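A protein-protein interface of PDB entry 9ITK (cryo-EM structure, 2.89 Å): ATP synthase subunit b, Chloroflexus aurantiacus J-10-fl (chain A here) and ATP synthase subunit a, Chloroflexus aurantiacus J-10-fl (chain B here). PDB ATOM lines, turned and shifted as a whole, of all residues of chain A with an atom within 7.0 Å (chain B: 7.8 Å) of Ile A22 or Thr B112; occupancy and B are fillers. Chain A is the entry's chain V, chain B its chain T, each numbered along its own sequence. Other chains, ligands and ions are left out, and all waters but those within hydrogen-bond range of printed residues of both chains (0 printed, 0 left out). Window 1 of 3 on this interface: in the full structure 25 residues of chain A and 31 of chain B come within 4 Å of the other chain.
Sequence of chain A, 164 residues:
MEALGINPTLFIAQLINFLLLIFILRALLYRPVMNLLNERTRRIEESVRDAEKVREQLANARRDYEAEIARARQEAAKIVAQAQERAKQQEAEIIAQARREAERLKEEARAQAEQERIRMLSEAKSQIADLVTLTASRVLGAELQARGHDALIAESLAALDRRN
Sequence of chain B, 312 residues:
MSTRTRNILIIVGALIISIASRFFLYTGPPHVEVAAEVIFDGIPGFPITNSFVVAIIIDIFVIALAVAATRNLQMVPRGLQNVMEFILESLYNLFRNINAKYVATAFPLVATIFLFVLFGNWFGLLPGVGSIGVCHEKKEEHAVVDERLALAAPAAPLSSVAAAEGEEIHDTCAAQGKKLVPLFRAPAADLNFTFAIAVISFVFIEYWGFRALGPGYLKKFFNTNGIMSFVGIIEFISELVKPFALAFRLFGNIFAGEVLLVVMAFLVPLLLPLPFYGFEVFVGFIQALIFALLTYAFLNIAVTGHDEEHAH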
ATOM      1  N   ASN A  17       6.932 -26.106  31.808  1.00  0.00           N
ATOM      2  CA  ASN A  17       6.152 -25.211  30.960  1.00  0.00           C
ATOM      3  C   ASN A  17       6.914 -24.841  29.694  1.00  0.00           C
ATOM      4  O   ASN A  17       6.388 -24.963  28.583  1.00  0.00           O
ATOM      5  CB  ASN A  17       5.761 -23.956  31.738  1.00  0.00           C
ATOM      6  CG  ASN A  17       4.769 -23.090  30.986  1.00  0.00           C
ATOM      7  OD1 ASN A  17       5.098 -22.490  29.963  1.00  0.00           O
ATOM      8  ND2 ASN A  17       3.543 -23.023  31.492  1.00  0.00           N
ATOM      9  N   PHE A  18       8.165 -24.394  29.839  1.00  0.00           N
ATOM     10  CA  PHE A  18       8.923 -23.963  28.669  1.00  0.00           C
ATOM     11  C   PHE A  18       9.195 -25.115  27.714  1.00  0.00           C
ATOM     12  O   PHE A  18       9.239 -24.907  26.496  1.00  0.00           O
ATOM     13  CB  PHE A  18      10.234 -23.304  29.091  1.00  0.00           C
ATOM     14  CG  PHE A  18      10.889 -22.510  27.995  1.00  0.00           C
ATOM     15  CD1 PHE A  18      10.391 -21.273  27.626  1.00  0.00           C
ATOM     16  CD2 PHE A  18      12.003 -23.001  27.337  1.00  0.00           C
ATOM     17  CE1 PHE A  18      10.993 -20.541  26.619  1.00  0.00           C
ATOM     18  CE2 PHE A  18      12.608 -22.275  26.332  1.00  0.00           C
ATOM     19  CZ  PHE A  18      12.102 -21.043  25.972  1.00  0.00           C
ATOM     20  N   LEU A  19       9.384 -26.328  28.236  1.00  0.00           N
ATOM     21  CA  LEU A  19       9.519 -27.484  27.358  1.00  0.00           C
ATOM     22  C   LEU A  19       8.265 -27.671  26.516  1.00  0.00           C
ATOM     23  O   LEU A  19       8.347 -27.999  25.328  1.00  0.00           O
ATOM     24  CB  LEU A  19       9.815 -28.740  28.176  1.00  0.00           C
ATOM     25  CG  LEU A  19      11.258 -28.909  28.651  1.00  0.00           C
ATOM     26  CD1 LEU A  19      11.502 -30.333  29.122  1.00  0.00           C
ATOM     27  CD2 LEU A  19      12.234 -28.530  27.548  1.00  0.00           C
ATOM     28  N   LEU A  20       7.095 -27.461  27.118  1.00  0.00           N
ATOM     29  CA  LEU A  20       5.854 -27.472  26.353  1.00  0.00           C
ATOM     30  C   LEU A  20       5.790 -26.305  25.376  1.00  0.00           C
ATOM     31  O   LEU A  20       5.158 -26.419  24.320  1.00  0.00           O
ATOM     32  CB  LEU A  20       4.659 -27.446  27.308  1.00  0.00           C
ATOM     33  CG  LEU A  20       3.244 -27.585  26.744  1.00  0.00           C
ATOM     34  CD1 LEU A  20       2.392 -28.419  27.682  1.00  0.00           C
ATOM     35  CD2 LEU A  20       2.613 -26.218  26.538  1.00  0.00           C
ATOM     36  N   LEU A  21       6.430 -25.181  25.707  1.00  0.00           N
ATOM     37  CA  LEU A  21       6.377 -24.015  24.831  1.00  0.00           C
ATOM     38  C   LEU A  21       7.103 -24.266  23.516  1.00  0.00           C
ATOM     39  O   LEU A  21       6.634 -23.841  22.453  1.00  0.00           O
ATOM     40  CB  LEU A  21       6.962 -22.794  25.542  1.00  0.00           C
ATOM     41  CG  LEU A  21       6.285 -22.379  26.851  1.00  0.00           C
ATOM     42  CD1 LEU A  21       6.785 -21.025  27.329  1.00  0.00           C
ATOM     43  CD2 LEU A  21       4.774 -22.383  26.706  1.00  0.00           C
ATOM     44  N   ILE A  22       8.254 -24.941  23.561  1.00  0.00           N
ATOM     45  CA  ILE A  22       9.009 -25.169  22.332  1.00  0.00           C
ATOM     46  C   ILE A  22       8.311 -26.190  21.444  1.00  0.00           C
ATOM     47  O   ILE A  22       8.395 -26.110  20.212  1.00  0.00           O
ATOM     48  CB  ILE A  22      10.458 -25.589  22.649  1.00  0.00           C
ATOM     49  CG1 ILE A  22      10.520 -27.025  23.166  1.00  0.00           C
ATOM     50  CG2 ILE A  22      11.066 -24.653  23.674  1.00  0.00           C
ATOM     51  CD1 ILE A  22      11.922 -27.590  23.226  1.00  0.00           C
ATOM     52  N   PHE A  23       7.612 -27.162  22.037  1.00  0.00           N
ATOM     53  CA  PHE A  23       6.992 -28.214  21.240  1.00  0.00           C
ATOM     54  C   PHE A  23       5.801 -27.688  20.451  1.00  0.00           C
ATOM     55  O   PHE A  23       5.639 -28.018  19.271  1.00  0.00           O
ATOM     56  CB  PHE A  23       6.568 -29.375  22.138  1.00  0.00           C
ATOM     57  CG  PHE A  23       7.716 -30.183  22.668  1.00  0.00           C
ATOM     58  CD1 PHE A  23       8.819 -30.448  21.874  1.00  0.00           C
ATOM     59  CD2 PHE A  23       7.688 -30.687  23.958  1.00  0.00           C
ATOM     60  CE1 PHE A  23       9.875 -31.192  22.360  1.00  0.00           C
ATOM     61  CE2 PHE A  23       8.741 -31.432  24.449  1.00  0.00           C
ATOM     62  CZ  PHE A  23       9.836 -31.685  23.649  1.00  0.00           C
ATOM     63  N   ILE A  24       4.956 -26.871  21.081  1.00  0.00           N
ATOM     64  CA  ILE A  24       3.747 -26.405  20.411  1.00  0.00           C
ATOM     65  C   ILE A  24       4.091 -25.449  19.274  1.00  0.00           C
ATOM     66  O   ILE A  24       3.463 -25.484  18.210  1.00  0.00           O
ATOM     67  CB  ILE A  24       2.777 -25.771  21.426  1.00  0.00           C
ATOM     68  CG1 ILE A  24       3.454 -24.635  22.192  1.00  0.00           C
ATOM     69  CG2 ILE A  24       2.253 -26.826  22.387  1.00  0.00           C
ATOM     70  CD1 ILE A  24       2.506 -23.838  23.054  1.00  0.00           C
ATOM     71  N   LEU A  25       5.090 -24.586  19.471  1.00  0.00           N
ATOM     72  CA  LEU A  25       5.510 -23.699  18.390  1.00  0.00           C
ATOM     73  C   LEU A  25       6.189 -24.476  17.269  1.00  0.00           C
ATOM     74  O   LEU A  25       6.078 -24.104  16.095  1.00  0.00           O
ATOM     75  CB  LEU A  25       6.441 -22.607  18.919  1.00  0.00           C
ATOM     76  CG  LEU A  25       5.832 -21.355  19.557  1.00  0.00           C
ATOM     77  CD1 LEU A  25       5.026 -20.585  18.522  1.00  0.00           C
ATOM     78  CD2 LEU A  25       4.983 -21.666  20.778  1.00  0.00           C
ATOM     79  N   ARG A  26       6.903 -25.552  17.610  1.00  0.00           N
ATOM     80  CA  ARG A  26       7.571 -26.344  16.584  1.00  0.00           C
ATOM     81  C   ARG A  26       6.563 -26.967  15.628  1.00  0.00           C
ATOM     82  O   ARG A  26       6.758 -26.945  14.409  1.00  0.00           O
ATOM     83  CB  ARG A  26       8.433 -27.426  17.232  1.00  0.00           C
ATOM     84  CG  ARG A  26       9.104 -28.360  16.238  1.00  0.00           C
ATOM     85  CD  ARG A  26      10.011 -29.348  16.947  1.00  0.00           C
ATOM     86  NE  ARG A  26      10.619 -30.299  16.024  1.00  0.00           N
ATOM     87  CZ  ARG A  26      11.500 -31.224  16.377  1.00  0.00           C
ATOM     88  NH1 ARG A  26      11.902 -31.353  17.632  1.00  0.00           N
ATOM     89  NH2 ARG A  26      11.994 -32.039  15.450  1.00  0.00           N
ATOM     90  N   ALA A  27       5.470 -27.512  16.161  1.00  0.00           N
ATOM     91  CA  ALA A  27       4.446 -28.125  15.329  1.00  0.00           C
ATOM     92  C   ALA A  27       3.491 -27.110  14.716  1.00  0.00           C
ATOM     93  O   ALA A  27       2.656 -27.492  13.889  1.00  0.00           O
ATOM     94  CB  ALA A  27       3.649 -29.147  16.144  1.00  0.00           C
ATOM     95  N   TYR A  30       7.386 -23.448  13.159  1.00  0.00           N
ATOM     96  CA  TYR A  30       8.747 -23.660  12.677  1.00  0.00           C
ATOM     97  C   TYR A  30       8.779 -24.612  11.487  1.00  0.00           C
ATOM     98  O   TYR A  30       9.422 -24.325  10.470  1.00  0.00           O
ATOM     99  CB  TYR A  30       9.627 -24.177  13.812  1.00  0.00           C
ATOM    100  CG  TYR A  30       9.807 -23.163  14.913  1.00  0.00           C
ATOM    101  CD1 TYR A  30       9.538 -21.821  14.689  1.00  0.00           C
ATOM    102  CD2 TYR A  30      10.233 -23.545  16.176  1.00  0.00           C
ATOM    103  CE1 TYR A  30       9.689 -20.889  15.685  1.00  0.00           C
ATOM    104  CE2 TYR A  30      10.389 -22.618  17.180  1.00  0.00           C
ATOM    105  CZ  TYR A  30      10.113 -21.291  16.929  1.00  0.00           C
ATOM    106  OH  TYR A  30      10.264 -20.354  17.922  1.00  0.00           O
ATOM    107  N   ASP B  59       3.325 -16.043  26.069  1.00  0.00           N
ATOM    108  CA  ASP B  59       3.093 -17.247  25.281  1.00  0.00           C
ATOM    109  C   ASP B  59       1.819 -17.128  24.457  1.00  0.00           C
ATOM    110  O   ASP B  59       1.788 -17.527  23.287  1.00  0.00           O
ATOM    111  CB  ASP B  59       3.024 -18.469  26.195  1.00  0.00           C
ATOM    112  CG  ASP B  59       2.910 -19.763  25.422  1.00  0.00           C
ATOM    113  OD1 ASP B  59       3.514 -19.860  24.333  1.00  0.00           O
ATOM    114  OD2 ASP B  59       2.207 -20.679  25.895  1.00  0.00           O
ATOM    115  N   VAL B  62       2.677 -14.930  21.724  1.00  0.00           N
ATOM    116  CA  VAL B  62       3.484 -15.673  20.759  1.00  0.00           C
ATOM    117  C   VAL B  62       2.606 -16.627  19.958  1.00  0.00           C
ATOM    118  O   VAL B  62       2.720 -16.722  18.731  1.00  0.00           O
ATOM    119  CB  VAL B  62       4.626 -16.418  21.474  1.00  0.00           C
ATOM    120  CG1 VAL B  62       5.149 -17.555  20.612  1.00  0.00           C
ATOM    121  CG2 VAL B  62       5.748 -15.453  21.818  1.00  0.00           C
ATOM    122  N   LEU B  88      12.407 -15.179  11.222  1.00  0.00           N
ATOM    123  CA  LEU B  88      12.845 -16.567  11.334  1.00  0.00           C
ATOM    124  C   LEU B  88      14.062 -16.846  10.459  1.00  0.00           C
ATOM    125  O   LEU B  88      14.994 -17.530  10.895  1.00  0.00           O
ATOM    126  CB  LEU B  88      11.698 -17.514  10.983  1.00  0.00           C
ATOM    127  CG  LEU B  88      10.794 -17.977  12.131  1.00  0.00           C
ATOM    128  CD1 LEU B  88      11.586 -18.797  13.127  1.00  0.00           C
ATOM    129  CD2 LEU B  88      10.112 -16.814  12.830  1.00  0.00           C
ATOM    130  N   PHE B  95      22.412 -18.786  12.786  1.00  0.00           N
ATOM    131  CA  PHE B  95      22.825 -20.070  13.339  1.00  0.00           C
ATOM    132  C   PHE B  95      23.553 -20.910  12.299  1.00  0.00           C
ATOM    133  O   PHE B  95      24.473 -21.665  12.636  1.00  0.00           O
ATOM    134  CB  PHE B  95      21.610 -20.817  13.886  1.00  0.00           C
ATOM    135  CG  PHE B  95      20.865 -20.056  14.938  1.00  0.00           C
ATOM    136  CD1 PHE B  95      21.543 -19.454  15.983  1.00  0.00           C
ATOM    137  CD2 PHE B  95      19.490 -19.933  14.880  1.00  0.00           C
ATOM    138  CE1 PHE B  95      20.860 -18.748  16.950  1.00  0.00           C
ATOM    139  CE2 PHE B  95      18.802 -19.224  15.842  1.00  0.00           C
ATOM    140  CZ  PHE B  95      19.488 -18.633  16.880  1.00  0.00           C
ATOM    141  N   ALA B 106      18.621 -27.889  16.468  1.00  0.00           N
ATOM    142  CA  ALA B 106      18.543 -27.002  17.619  1.00  0.00           C
ATOM    143  C   ALA B 106      17.655 -25.789  17.384  1.00  0.00           C
ATOM    144  O   ALA B 106      17.462 -24.998  18.313  1.00  0.00           O
ATOM    145  CB  ALA B 106      19.946 -26.535  18.019  1.00  0.00           C
ATOM    146  N   PHE B 107      17.117 -25.622  16.178  1.00  0.00           N
ATOM    147  CA  PHE B 107      16.316 -24.435  15.889  1.00  0.00           C
ATOM    148  C   PHE B 107      15.086 -24.278  16.775  1.00  0.00           C
ATOM    149  O   PHE B 107      14.839 -23.149  17.232  1.00  0.00           O
ATOM    150  CB  PHE B 107      15.898 -24.418  14.417  1.00  0.00           C
ATOM    151  CG  PHE B 107      15.456 -23.072  13.940  1.00  0.00           C
ATOM    152  CD1 PHE B 107      16.380 -22.071  13.708  1.00  0.00           C
ATOM    153  CD2 PHE B 107      14.117 -22.799  13.745  1.00  0.00           C
ATOM    154  CE1 PHE B 107      15.976 -20.827  13.275  1.00  0.00           C
ATOM    155  CE2 PHE B 107      13.708 -21.559  13.313  1.00  0.00           C
ATOM    156  CZ  PHE B 107      14.639 -20.571  13.077  1.00  0.00           C
ATOM    157  N   PRO B 108      14.269 -25.310  17.031  1.00  0.00           N
ATOM    158  CA  PRO B 108      13.072 -25.077  17.858  1.00  0.00           C
ATOM    159  C   PRO B 108      13.387 -24.507  19.227  1.00  0.00           C
ATOM    160  O   PRO B 108      12.635 -23.661  19.724  1.00  0.00           O
ATOM    161  CB  PRO B 108      12.434 -26.470  17.953  1.00  0.00           C
ATOM    162  CG  PRO B 108      12.931 -27.199  16.770  1.00  0.00           C
ATOM    163  CD  PRO B 108      14.313 -26.692  16.518  1.00  0.00           C
ATOM    164  N   LEU B 109      14.483 -24.935  19.852  1.00  0.00           N
ATOM    165  CA  LEU B 109      14.834 -24.393  21.160  1.00  0.00           C
ATOM    166  C   LEU B 109      15.231 -22.925  21.066  1.00  0.00           C
ATOM    167  O   LEU B 109      14.692 -22.079  21.788  1.00  0.00           O
ATOM    168  CB  LEU B 109      15.964 -25.212  21.781  1.00  0.00           C
ATOM    169  CG  LEU B 109      16.570 -24.605  23.046  1.00  0.00           C
ATOM    170  CD1 LEU B 109      15.535 -24.522  24.153  1.00  0.00           C
ATOM    171  CD2 LEU B 109      17.775 -25.403  23.494  1.00  0.00           C
ATOM    172  N   VAL B 110      16.161 -22.599  20.165  1.00  0.00           N
ATOM    173  CA  VAL B 110      16.720 -21.252  20.135  1.00  0.00           C
ATOM    174  C   VAL B 110      15.698 -20.248  19.616  1.00  0.00           C
ATOM    175  O   VAL B 110      15.605 -19.122  20.120  1.00  0.00           O
ATOM    176  CB  VAL B 110      18.019 -21.227  19.309  1.00  0.00           C
ATOM    177  CG1 VAL B 110      19.113 -21.978  20.035  1.00  0.00           C
ATOM    178  CG2 VAL B 110      17.795 -21.830  17.945  1.00  0.00           C
ATOM    179  N   ALA B 111      14.924 -20.627  18.597  1.00  0.00           N
ATOM    180  CA  ALA B 111      13.941 -19.703  18.042  1.00  0.00           C
ATOM    181  C   ALA B 111      12.862 -19.367  19.064  1.00  0.00           C
ATOM    182  O   ALA B 111      12.429 -18.214  19.162  1.00  0.00           O
ATOM    183  CB  ALA B 111      13.327 -20.287  16.770  1.00  0.00           C
ATOM    184  N   THR B 112      12.408 -20.360  19.831  1.00  0.00           N
ATOM    185  CA  THR B 112      11.513 -20.070  20.947  1.00  0.00           C
ATOM    186  C   THR B 112      12.204 -19.210  21.995  1.00  0.00           C
ATOM    187  O   THR B 112      11.582 -18.318  22.584  1.00  0.00           O
ATOM    188  CB  THR B 112      11.005 -21.366  21.572  1.00  0.00           C
ATOM    189  OG1 THR B 112      12.123 -22.170  21.968  1.00  0.00           O
ATOM    190  CG2 THR B 112      10.102 -22.128  20.610  1.00  0.00           C
ATOM    191  N   ILE B 113      13.487 -19.473  22.252  1.00  0.00           N
ATOM    192  CA  ILE B 113      14.231 -18.662  23.213  1.00  0.00           C
ATOM    193  C   ILE B 113      14.261 -17.206  22.769  1.00  0.00           C
ATOM    194  O   ILE B 113      13.973 -16.294  23.550  1.00  0.00           O
ATOM    195  CB  ILE B 113      15.651 -19.224  23.408  1.00  0.00           C
ATOM    196  CG1 ILE B 113      15.645 -20.421  24.356  1.00  0.00           C
ATOM    197  CG2 ILE B 113      16.590 -18.159  23.915  1.00  0.00           C
ATOM    198  CD1 ILE B 113      17.033 -20.944  24.654  1.00  0.00           C
ATOM    199  N   PHE B 114      14.589 -16.969  21.497  1.00  0.00           N
ATOM    200  CA  PHE B 114      14.692 -15.599  21.005  1.00  0.00           C
ATOM    201  C   PHE B 114      13.341 -14.894  21.031  1.00  0.00           C
ATOM    202  O   PHE B 114      13.245 -13.734  21.444  1.00  0.00           O
ATOM    203  CB  PHE B 114      15.273 -15.592  19.593  1.00  0.00           C
ATOM    204  CG  PHE B 114      15.306 -14.234  18.963  1.00  0.00           C
ATOM    205  CD1 PHE B 114      16.193 -13.275  19.410  1.00  0.00           C
ATOM    206  CD2 PHE B 114      14.451 -13.915  17.926  1.00  0.00           C
ATOM    207  CE1 PHE B 114      16.228 -12.025  18.835  1.00  0.00           C
ATOM    208  CE2 PHE B 114      14.482 -12.667  17.348  1.00  0.00           C
ATOM    209  CZ  PHE B 114      15.372 -11.723  17.801  1.00  0.00           C
ATOM    210  N   LEU B 115      12.281 -15.580  20.595  1.00  0.00           N
ATOM    211  CA  LEU B 115      10.978 -14.928  20.494  1.00  0.00           C
ATOM    212  C   LEU B 115      10.338 -14.722  21.862  1.00  0.00           C
ATOM    213  O   LEU B 115       9.737 -13.671  22.117  1.00  0.00           O
ATOM    214  CB  LEU B 115      10.046 -15.735  19.590  1.00  0.00           C
ATOM    215  CG  LEU B 115      10.060 -15.459  18.084  1.00  0.00           C
ATOM    216  CD1 LEU B 115       9.590 -14.042  17.805  1.00  0.00           C
ATOM    217  CD2 LEU B 115      11.424 -15.701  17.467  1.00  0.00           C
ATOM    218  N   PHE B 116      10.444 -15.708  22.753  1.00  0.00           N
ATOM    219  CA  PHE B 116       9.710 -15.634  24.012  1.00  0.00           C
ATOM    220  C   PHE B 116      10.253 -14.532  24.914  1.00  0.00           C
ATOM    221  O   PHE B 116       9.487 -13.725  25.453  1.00  0.00           O
ATOM    222  CB  PHE B 116       9.751 -16.981  24.731  1.00  0.00           C
ATOM    223  CG  PHE B 116       8.888 -17.033  25.956  1.00  0.00           C
ATOM    224  CD1 PHE B 116       7.510 -17.116  25.841  1.00  0.00           C
ATOM    225  CD2 PHE B 116       9.449 -16.990  27.219  1.00  0.00           C
ATOM    226  CE1 PHE B 116       6.710 -17.160  26.962  1.00  0.00           C
ATOM    227  CE2 PHE B 116       8.652 -17.032  28.342  1.00  0.00           C
ATOM    228  CZ  PHE B 116       7.283 -17.119  28.215  1.00  0.00           C
ATOM    229  N   VAL B 117      11.574 -14.479  25.092  1.00  0.00           N
ATOM    230  CA  VAL B 117      12.127 -13.523  26.045  1.00  0.00           C
ATOM    231  C   VAL B 117      12.177 -12.119  25.455  1.00  0.00           C
ATOM    232  O   VAL B 117      12.187 -11.134  26.202  1.00  0.00           O
ATOM    233  CB  VAL B 117      13.517 -13.972  26.531  1.00  0.00           C
ATOM    234  CG1 VAL B 117      13.454 -15.376  27.110  1.00  0.00           C
ATOM    235  CG2 VAL B 117      14.533 -13.890  25.414  1.00  0.00           C
ATOM    236  N   LEU B 118      12.209 -11.991  24.126  1.00  0.00           N
ATOM    237  CA  LEU B 118      12.208 -10.664  23.517  1.00  0.00           C
ATOM    238  C   LEU B 118      10.921  -9.920  23.839  1.00  0.00           C
ATOM    239  O   LEU B 118      10.951  -8.781  24.317  1.00  0.00           O
ATOM    240  CB  LEU B 118      12.397 -10.777  22.004  1.00  0.00           C
ATOM    241  CG  LEU B 118      12.694  -9.494  21.220  1.00  0.00           C
ATOM    242  CD1 LEU B 118      13.501  -9.820  19.982  1.00  0.00           C
ATOM    243  CD2 LEU B 118      11.422  -8.763  20.824  1.00  0.00           C
ATOM    244  N   PHE B 193      12.639 -18.296  36.495  1.00  0.00           N
ATOM    245  CA  PHE B 193      12.446 -18.481  35.061  1.00  0.00           C
ATOM    246  C   PHE B 193      13.780 -18.603  34.338  1.00  0.00           C
ATOM    247  O   PHE B 193      13.997 -19.549  33.573  1.00  0.00           O
ATOM    248  CB  PHE B 193      11.625 -17.321  34.498  1.00  0.00           C
ATOM    249  CG  PHE B 193      11.608 -17.253  32.996  1.00  0.00           C
ATOM    250  CD1 PHE B 193      10.726 -18.030  32.268  1.00  0.00           C
ATOM    251  CD2 PHE B 193      12.460 -16.403  32.313  1.00  0.00           C
ATOM    252  CE1 PHE B 193      10.702 -17.965  30.890  1.00  0.00           C
ATOM    253  CE2 PHE B 193      12.440 -16.333  30.936  1.00  0.00           C
ATOM    254  CZ  PHE B 193      11.560 -17.115  30.223  1.00  0.00           C
ATOM    255  N   ILE B 197      15.188 -21.631  32.181  1.00  0.00           N
ATOM    256  CA  ILE B 197      15.518 -21.578  30.761  1.00  0.00           C
ATOM    257  C   ILE B 197      16.953 -22.025  30.530  1.00  0.00           C
ATOM    258  O   ILE B 197      17.244 -22.758  29.578  1.00  0.00           O
ATOM    259  CB  ILE B 197      15.272 -20.166  30.203  1.00  0.00           C
ATOM    260  CG1 ILE B 197      13.848 -19.718  30.507  1.00  0.00           C
ATOM    261  CG2 ILE B 197      15.479 -20.154  28.708  1.00  0.00           C
ATOM    262  CD1 ILE B 197      12.801 -20.711  30.094  1.00  0.00           C
ATOM    263  N   ILE B 200      17.350 -25.747  30.707  1.00  0.00           N
ATOM    264  CA  ILE B 200      16.871 -26.277  29.433  1.00  0.00           C
ATOM    265  C   ILE B 200      17.920 -26.062  28.356  1.00  0.00           C
ATOM    266  O   ILE B 200      18.216 -26.964  27.563  1.00  0.00           O
ATOM    267  CB  ILE B 200      15.531 -25.628  29.043  1.00  0.00           C
ATOM    268  CG1 ILE B 200      14.455 -25.969  30.067  1.00  0.00           C
ATOM    269  CG2 ILE B 200      15.106 -26.074  27.655  1.00  0.00           C
ATOM    270  CD1 ILE B 200      13.188 -25.175  29.906  1.00  0.00           C
ATOM    271  N   PHE B 204      20.353 -29.217  26.810  1.00  0.00           N
ATOM    272  CA  PHE B 204      20.365 -29.405  25.366  1.00  0.00           C
ATOM    273  C   PHE B 204      21.786 -29.461  24.821  1.00  0.00           C
ATOM    274  O   PHE B 204      21.998 -29.913  23.691  1.00  0.00           O
ATOM    275  CB  PHE B 204      19.579 -28.276  24.701  1.00  0.00           C
ATOM    276  CG  PHE B 204      19.137 -28.577  23.298  1.00  0.00           C
ATOM    277  CD1 PHE B 204      17.941 -29.232  23.062  1.00  0.00           C
ATOM    278  CD2 PHE B 204      19.900 -28.178  22.218  1.00  0.00           C
ATOM    279  CE1 PHE B 204      17.523 -29.498  21.773  1.00  0.00           C
ATOM    280  CE2 PHE B 204      19.488 -28.442  20.927  1.00  0.00           C
ATOM    281  CZ  PHE B 204      18.298 -29.100  20.704  1.00  0.00           C
ATOM    282  N   ALA B 292      19.951 -16.929  22.903  1.00  0.00           N
ATOM    283  CA  ALA B 292      19.803 -17.974  21.898  1.00  0.00           C
ATOM    284  C   ALA B 292      21.119 -18.221  21.172  1.00  0.00           C
ATOM    285  O   ALA B 292      21.474 -19.371  20.889  1.00  0.00           O
ATOM    286  CB  ALA B 292      18.706 -17.595  20.904  1.00  0.00           C
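Hydrophobic or aromatic side chains of chain B that line the printed part of chain A: Val B62, Leu B88, Pro B108, Ala B111, Ile B113, Phe B116, Ile B197 and Ile B200. Of the 12 printed residues of chain A, 7 touch a printed residue of chain B. Printed residues of chain A that touch a printed residue of chain B: Phe A18, Leu A19, Leu A21, Ile A22, Leu A25, Arg A26 and Tyr A30. Hydrophobic or aromatic side chains of chain A that line the printed part of chain B: Phe A18, Leu A19, Leu A21, Ile A22, Leu A25 and Tyr A30. Among the printed residues, 14 pairs touch across the chains.
The backbone carbonyl oxygen (O) of Leu A25 is in hydrogen-bond range of the backbone NH (N) of Tyr A30 (3.3 Å). The side-chain hydroxyl of Thr B112 lies within hydrogen-bond range of the backbone carbonyl oxygen of Pro B108 (2.7 Å). The backbone carbonyl oxygen (O) of Leu B109 sits at hydrogen-bond distance from the side-chain hydroxyl (OG1) of Thr B112.
Among the printed residues, merely in contact across the chains: Leu A21 with Asp B59 (3.2 Å), Ile A22 with Thr B112 (3.2 Å), Phe A18 with Ile B197 (3.4 Å), Tyr A30 with Pro B108 (3.6 Å), Phe A18 with Ile B200 (3.6 Å), Arg A26 with Pro B108 (3.6 Å), Leu A25 with Val B62 (3.7 Å), Leu A19 with Ile B200 (3.8 Å), Tyr A30 with Leu B88 (3.8 Å), Leu A21 with Phe B116 (3.9 Å), Phe A18 with Phe B116 (3.9 Å) and Phe A18 with Ile B113 (3.9 Å).
Of chain B, only Thr B112 comes within 4 Å of Ile A22. Thr B112 touches just these residues of chain A: Ile A22 and Tyr A30. Printed residues of chain A within 4 Å of Val B62: Leu A25. Printed residues of chain B within 4 Å of Leu A25: Val B62. Phe B114 touches none of the printed residues of chain A. The nearest residue of chain B that does not touch Ile A22 is Pro B108 (4.1 Å). The nearest residue of chain A that does not touch Thr B112 is Leu A25 (4.1 Å).
The backbone NH of Thr B112 lies within hydrogen-bond range of the side-chain hydroxyl of Tyr A30. The side-chain hydroxyl of Tyr A30 lies close to the backbone carbonyl oxygen of Ala B111.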
